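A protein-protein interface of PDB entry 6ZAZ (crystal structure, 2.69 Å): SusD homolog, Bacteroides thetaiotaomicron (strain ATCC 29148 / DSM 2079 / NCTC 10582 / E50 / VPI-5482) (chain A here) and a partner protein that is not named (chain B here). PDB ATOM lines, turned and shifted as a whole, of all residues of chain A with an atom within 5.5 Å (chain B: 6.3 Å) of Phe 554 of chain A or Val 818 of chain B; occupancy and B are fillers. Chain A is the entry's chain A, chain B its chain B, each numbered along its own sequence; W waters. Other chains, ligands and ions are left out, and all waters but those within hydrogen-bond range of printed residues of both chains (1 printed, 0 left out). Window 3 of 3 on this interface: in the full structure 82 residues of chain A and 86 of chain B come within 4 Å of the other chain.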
ATOM      1  N   THR A 100      -4.132   0.140  22.688  1.00  0.00           N
ATOM      2  CA  THR A 100      -3.123  -0.816  23.132  1.00  0.00           C
ATOM      3  C   THR A 100      -2.692  -0.558  24.570  1.00  0.00           C
ATOM      4  O   THR A 100      -2.058  -1.428  25.182  1.00  0.00           O
ATOM      5  CB  THR A 100      -1.904  -0.801  22.204  1.00  0.00           C
ATOM      6  OG1 THR A 100      -1.188   0.428  22.362  1.00  0.00           O
ATOM      7  CG2 THR A 100      -2.322  -0.969  20.750  1.00  0.00           C
ATOM      8  N   THR A 101      -3.055   0.596  25.128  1.00  0.00           N
ATOM      9  CA  THR A 101      -2.747   0.942  26.507  1.00  0.00           C
ATOM     10  C   THR A 101      -3.816   0.486  27.501  1.00  0.00           C
ATOM     11  O   THR A 101      -3.723   0.830  28.685  1.00  0.00           O
ATOM     12  CB  THR A 101      -2.535   2.458  26.629  1.00  0.00           C
ATOM     13  OG1 THR A 101      -3.562   3.170  25.919  1.00  0.00           O
ATOM     14  CG2 THR A 101      -1.200   2.839  26.061  1.00  0.00           C
ATOM     15  N   VAL A 552      -0.823  -6.694  21.495  1.00  0.00           N
ATOM     16  CA  VAL A 552       0.134  -6.899  22.583  1.00  0.00           C
ATOM     17  C   VAL A 552       0.114  -5.650  23.450  1.00  0.00           C
ATOM     18  O   VAL A 552      -0.069  -4.540  22.914  1.00  0.00           O
ATOM     19  CB  VAL A 552       1.535  -7.166  22.014  1.00  0.00           C
ATOM     20  CG1 VAL A 552       2.594  -7.138  23.124  1.00  0.00           C
ATOM     21  CG2 VAL A 552       1.554  -8.460  21.241  1.00  0.00           C
ATOM     22  N   PRO A 553       0.210  -5.742  24.776  1.00  0.00           N
ATOM     23  CA  PRO A 553      -0.020  -4.542  25.597  1.00  0.00           C
ATOM     24  C   PRO A 553       1.036  -3.482  25.350  1.00  0.00           C
ATOM     25  O   PRO A 553       2.212  -3.793  25.143  1.00  0.00           O
ATOM     26  CB  PRO A 553       0.045  -5.067  27.031  1.00  0.00           C
ATOM     27  CG  PRO A 553      -0.354  -6.505  26.893  1.00  0.00           C
ATOM     28  CD  PRO A 553       0.245  -6.965  25.598  1.00  0.00           C
ATOM     29  N   PHE A 554       0.609  -2.213  25.376  1.00  0.00           N
ATOM     30  CA  PHE A 554       1.560  -1.145  25.074  1.00  0.00           C
ATOM     31  C   PHE A 554       2.714  -1.129  26.070  1.00  0.00           C
ATOM     32  O   PHE A 554       3.881  -1.165  25.676  1.00  0.00           O
ATOM     33  CB  PHE A 554       0.882   0.219  25.025  1.00  0.00           C
ATOM     34  CG  PHE A 554       1.858   1.356  24.843  1.00  0.00           C
ATOM     35  CD1 PHE A 554       2.149   1.832  23.586  1.00  0.00           C
ATOM     36  CD2 PHE A 554       2.480   1.950  25.934  1.00  0.00           C
ATOM     37  CE1 PHE A 554       3.045   2.853  23.416  1.00  0.00           C
ATOM     38  CE2 PHE A 554       3.376   2.979  25.759  1.00  0.00           C
ATOM     39  CZ  PHE A 554       3.655   3.424  24.502  1.00  0.00           C
ATOM     40  N   GLU A 555       2.408  -1.047  27.370  1.00  0.00           N
ATOM     41  CA  GLU A 555       3.474  -1.077  28.370  1.00  0.00           C
ATOM     42  C   GLU A 555       4.406  -2.269  28.177  1.00  0.00           C
ATOM     43  O   GLU A 555       5.610  -2.152  28.418  1.00  0.00           O
ATOM     44  CB  GLU A 555       2.890  -1.085  29.780  1.00  0.00           C
ATOM     45  CG  GLU A 555       3.915  -1.262  30.887  1.00  0.00           C
ATOM     46  CD  GLU A 555       3.265  -1.370  32.270  1.00  0.00           C
ATOM     47  OE1 GLU A 555       2.009  -1.351  32.341  1.00  0.00           O
ATOM     48  OE2 GLU A 555       4.002  -1.460  33.281  1.00  0.00           O
ATOM     49  N   GLN A 556       3.889  -3.409  27.704  1.00  0.00           N
ATOM     50  CA  GLN A 556       4.759  -4.566  27.521  1.00  0.00           C
ATOM     51  C   GLN A 556       5.760  -4.331  26.390  1.00  0.00           C
ATOM     52  O   GLN A 556       6.971  -4.476  26.590  1.00  0.00           O
ATOM     53  CB  GLN A 556       3.933  -5.836  27.284  1.00  0.00           C
ATOM     54  CG  GLN A 556       3.129  -6.294  28.506  1.00  0.00           C
ATOM     55  CD  GLN A 556       3.960  -6.414  29.786  1.00  0.00           C
ATOM     56  OE1 GLN A 556       5.018  -7.046  29.797  1.00  0.00           O
ATOM     57  NE2 GLN A 556       3.472  -5.814  30.868  1.00  0.00           N
ATOM     58  N   ILE A 557       5.274  -3.963  25.196  1.00  0.00           N
ATOM     59  CA  ILE A 557       6.168  -3.580  24.098  1.00  0.00           C
ATOM     60  C   ILE A 557       7.149  -2.518  24.564  1.00  0.00           C
ATOM     61  O   ILE A 557       8.360  -2.613  24.325  1.00  0.00           O
ATOM     62  CB  ILE A 557       5.368  -3.060  22.894  1.00  0.00           C
ATOM     63  CG1 ILE A 557       4.508  -4.147  22.282  1.00  0.00           C
ATOM     64  CG2 ILE A 557       6.310  -2.477  21.851  1.00  0.00           C
ATOM     65  CD1 ILE A 557       3.376  -3.588  21.479  1.00  0.00           C
ATOM     66  N   SER A 558       6.629  -1.478  25.221  1.00  0.00           N
ATOM     67  CA  SER A 558       7.437  -0.299  25.509  1.00  0.00           C
ATOM     68  C   SER A 558       8.579  -0.634  26.466  1.00  0.00           C
ATOM     69  O   SER A 558       9.676  -0.083  26.354  1.00  0.00           O
ATOM     70  CB  SER A 558       6.531   0.822  26.045  1.00  0.00           C
ATOM     71  OG  SER A 558       7.257   1.881  26.654  1.00  0.00           O
ATOM     72  N   ALA A 559       8.351  -1.553  27.399  1.00  0.00           N
ATOM     73  CA  ALA A 559       9.429  -1.965  28.288  1.00  0.00           C
ATOM     74  C   ALA A 559      10.436  -2.860  27.570  1.00  0.00           C
ATOM     75  O   ALA A 559      11.614  -2.902  27.946  1.00  0.00           O
ATOM     76  CB  ALA A 559       8.851  -2.675  29.515  1.00  0.00           C
ATOM     77  N   GLN A 566       4.442  -5.524  17.804  1.00  0.00           N
ATOM     78  CA  GLN A 566       2.993  -5.471  17.840  1.00  0.00           C
ATOM     79  C   GLN A 566       2.377  -6.324  16.717  1.00  0.00           C
ATOM     80  O   GLN A 566       3.010  -6.617  15.688  1.00  0.00           O
ATOM     81  CB  GLN A 566       2.530  -4.007  17.757  1.00  0.00           C
ATOM     82  CG  GLN A 566       1.012  -3.819  17.831  1.00  0.00           C
ATOM     83  CD  GLN A 566       0.416  -4.464  19.079  1.00  0.00           C
ATOM     84  OE1 GLN A 566      -0.188  -5.541  19.019  1.00  0.00           O
ATOM     85  NE2 GLN A 566       0.558  -3.789  20.205  1.00  0.00           N
ATOM     86  N   ALA A 573       3.047   2.927  17.945  1.00  0.00           N
ATOM     87  CA  ALA A 573       2.857   3.806  19.106  1.00  0.00           C
ATOM     88  C   ALA A 573       3.996   3.703  20.133  1.00  0.00           C
ATOM     89  O   ALA A 573       5.045   4.348  20.004  1.00  0.00           O
ATOM     90  CB  ALA A 573       1.517   3.497  19.769  1.00  0.00           C
ATOM     91  N   ALA B 808       9.731   3.166  34.077  1.00  0.00           N
ATOM     92  CA  ALA B 808       9.401   4.265  33.176  1.00  0.00           C
ATOM     93  C   ALA B 808       8.136   3.956  32.395  1.00  0.00           C
ATOM     94  O   ALA B 808       7.223   4.790  32.315  1.00  0.00           O
ATOM     95  CB  ALA B 808      10.563   4.547  32.229  1.00  0.00           C
ATOM     96  N   ALA B 809       8.069   2.753  31.814  1.00  0.00           N
ATOM     97  CA  ALA B 809       6.838   2.278  31.199  1.00  0.00           C
ATOM     98  C   ALA B 809       5.750   2.012  32.233  1.00  0.00           C
ATOM     99  O   ALA B 809       4.568   1.946  31.873  1.00  0.00           O
ATOM    100  CB  ALA B 809       7.114   1.005  30.406  1.00  0.00           C
ATOM    101  N   GLY B 811       4.585   3.899  34.721  1.00  0.00           N
ATOM    102  CA  GLY B 811       3.780   5.004  35.157  1.00  0.00           C
ATOM    103  C   GLY B 811       3.854   5.270  36.641  1.00  0.00           C
ATOM    104  O   GLY B 811       3.229   6.235  37.107  1.00  0.00           O
ATOM    105  N   GLY B 815       4.127   9.475  33.740  1.00  0.00           N
ATOM    106  CA  GLY B 815       3.235   9.605  32.604  1.00  0.00           C
ATOM    107  C   GLY B 815       2.353   8.440  32.211  1.00  0.00           C
ATOM    108  O   GLY B 815       2.368   8.012  31.047  1.00  0.00           O
ATOM    109  N   ASN B 816       1.597   7.923  33.188  1.00  0.00           N
ATOM    110  CA  ASN B 816       0.371   7.138  33.003  1.00  0.00           C
ATOM    111  C   ASN B 816       0.617   5.827  32.275  1.00  0.00           C
ATOM    112  O   ASN B 816      -0.327   5.211  31.731  1.00  0.00           O
ATOM    113  CB  ASN B 816      -0.713   7.957  32.281  1.00  0.00           C
ATOM    114  CG  ASN B 816      -1.017   9.284  32.993  1.00  0.00           C
ATOM    115  OD1 ASN B 816      -2.093   9.471  33.578  1.00  0.00           O
ATOM    116  ND2 ASN B 816      -0.052  10.206  32.951  1.00  0.00           N
ATOM    117  N   GLY B 817       1.868   5.375  32.288  1.00  0.00           N
ATOM    118  CA  GLY B 817       2.229   4.222  31.500  1.00  0.00           C
ATOM    119  C   GLY B 817       2.020   4.405  30.016  1.00  0.00           C
ATOM    120  O   GLY B 817       1.760   3.426  29.309  1.00  0.00           O
ATOM    121  N   VAL B 818       2.103   5.635  29.515  1.00  0.00           N
ATOM    122  CA  VAL B 818       2.145   5.864  28.082  1.00  0.00           C
ATOM    123  C   VAL B 818       3.439   6.547  27.654  1.00  0.00           C
ATOM    124  O   VAL B 818       4.029   6.164  26.640  1.00  0.00           O
ATOM    125  CB  VAL B 818       0.900   6.642  27.589  1.00  0.00           C
ATOM    126  CG1 VAL B 818      -0.357   6.099  28.257  1.00  0.00           C
ATOM    127  CG2 VAL B 818       1.026   8.116  27.796  1.00  0.00           C
ATOM    128  N   LYS B 819       3.933   7.511  28.441  1.00  0.00           N
ATOM    129  CA  LYS B 819       5.238   8.134  28.234  1.00  0.00           C
ATOM    130  C   LYS B 819       6.066   8.049  29.518  1.00  0.00           C
ATOM    131  O   LYS B 819       5.540   7.932  30.630  1.00  0.00           O
ATOM    132  CB  LYS B 819       5.118   9.613  27.782  1.00  0.00           C
ATOM    133  CG  LYS B 819       4.561   9.811  26.346  1.00  0.00           C
ATOM    134  CD  LYS B 819       4.432  11.312  25.982  1.00  0.00           C
ATOM    135  CE  LYS B 819       4.556  11.605  24.474  1.00  0.00           C
ATOM    136  NZ  LYS B 819       3.507  10.917  23.655  1.00  0.00           N
ATOM    137  N   SER B 820       7.380   8.114  29.350  1.00  0.00           N
ATOM    138  CA  SER B 820       8.297   7.957  30.465  1.00  0.00           C
ATOM    139  C   SER B 820       8.504   9.291  31.173  1.00  0.00           C
ATOM    140  O   SER B 820       8.701  10.317  30.522  1.00  0.00           O
ATOM    141  CB  SER B 820       9.621   7.400  29.958  1.00  0.00           C
ATOM    142  OG  SER B 820      10.688   7.621  30.854  1.00  0.00           O
ATOM    143  N   VAL B 830       0.301  12.605  31.720  1.00  0.00           N
ATOM    144  CA  VAL B 830       0.194  12.719  30.272  1.00  0.00           C
ATOM    145  C   VAL B 830      -1.260  12.478  29.884  1.00  0.00           C
ATOM    146  O   VAL B 830      -1.934  11.628  30.477  1.00  0.00           O
ATOM    147  CB  VAL B 830       1.146  11.703  29.592  1.00  0.00           C
ATOM    148  CG1 VAL B 830       0.642  11.311  28.233  1.00  0.00           C
ATOM    149  CG2 VAL B 830       2.538  12.289  29.476  1.00  0.00           C
ATOM    150  N   GLY B 831      -1.757  13.232  28.907  1.00  0.00           N
ATOM    151  CA  GLY B 831      -3.141  13.009  28.529  1.00  0.00           C
ATOM    152  C   GLY B 831      -3.503  13.616  27.195  1.00  0.00           C
ATOM    153  O   GLY B 831      -2.682  14.253  26.532  1.00  0.00           O
ATOM    154  N   GLU B 871      -4.747   6.771  20.352  1.00  0.00           N
ATOM    155  CA  GLU B 871      -4.010   6.757  21.609  1.00  0.00           C
ATOM    156  C   GLU B 871      -2.680   7.485  21.536  1.00  0.00           C
ATOM    157  O   GLU B 871      -2.071   7.710  22.583  1.00  0.00           O
ATOM    158  CB  GLU B 871      -3.797   5.311  22.054  1.00  0.00           C
ATOM    159  CG  GLU B 871      -2.459   4.713  21.704  1.00  0.00           C
ATOM    160  CD  GLU B 871      -2.441   3.226  21.961  1.00  0.00           C
ATOM    161  OE1 GLU B 871      -3.505   2.591  21.812  1.00  0.00           O
ATOM    162  OE2 GLU B 871      -1.371   2.692  22.314  1.00  0.00           O
ATOM    163  N   GLN B 874      -1.537  12.136  22.877  1.00  0.00           N
ATOM    164  CA  GLN B 874      -1.462  12.580  24.264  1.00  0.00           C
ATOM    165  C   GLN B 874      -0.127  13.260  24.522  1.00  0.00           C
ATOM    166  O   GLN B 874       0.867  13.014  23.837  1.00  0.00           O
ATOM    167  CB  GLN B 874      -1.640  11.432  25.255  1.00  0.00           C
ATOM    168  CG  GLN B 874      -2.695  10.410  24.882  1.00  0.00           C
ATOM    169  CD  GLN B 874      -2.850   9.384  25.969  1.00  0.00           C
ATOM    170  OE1 GLN B 874      -2.712   9.716  27.146  1.00  0.00           O
ATOM    171  NE2 GLN B 874      -3.128   8.134  25.598  1.00  0.00           N
HETATM  172  O   HOH W   1      -1.918   3.171  29.904  1.00  0.00           O
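N of Thr 100 of chain A is in hydrogen-bond range of OE1 of Glu 871 of chain B (2.7 Å).
The backbone NH (N) of Phe 554 of chain A is in hydrogen-bond range of the backbone carbonyl oxygen (O) of Thr 100 of chain A (2.8 Å). The backbone carbonyl oxygen of Glu 871 of chain B is in hydrogen-bond range of the side-chain amide nitrogen of Gln 874 of chain B, at 3.2 Å.
Thr 101 of chain A touches Glu 871 of chain B. Phe 554 of chain A touches Gly 817 of chain B. Phe 554 of chain A touches Val 818 of chain B. Phe 554 of chain A touches Glu 871 of chain B. Ala 809 of chain B touches Glu 555 of chain A. Ser 558 of chain A touches Ala 809 of chain B. OE2 of Glu 871 of chain B touches CB of Ala 573 of chain A, 3.9 Å away.
Printed residues of chain B within 4 Å of Thr 100 of chain A: Glu 871. Of the printed residues of chain B, Thr 101 of chain A touches Glu 871 (3.8 Å). Pro 553 of chain A touches none of the printed residues of chain B. Phe 554 of chain A touches just these residues of chain B: Gly 817, Val 818 and Glu 871. Of the printed residues of chain B, Glu 555 of chain A touches Ala 809. Gln 566 of chain A touches none of the printed residues of chain B. Of the printed residues of chain B, Ala 573 of chain A touches Glu 871 (3.9 Å). Printed residues of chain A within 4 Å of Gly 817 of chain B: Phe 554. Val 818 of chain B touches just one residue of chain A: Phe 554 (3.4 Å). The nearest residue of chain B that does not touch Phe 554 of chain A is Lys 819 of chain B (5.3 Å). The nearest printed residue of chain B that does not touch Ala 573 of chain A is Val 818 of chain B (7.0 Å).
Hydrophobic or aromatic side chains of chain B within 4 Å of the printed part of chain A: Ala 809. Along chain B the printed residues that touch a printed residue of chain A span positions 809 to 871.
Water W1 bridges O of Asn 816 of chain B and O of Thr 101 of chain A.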
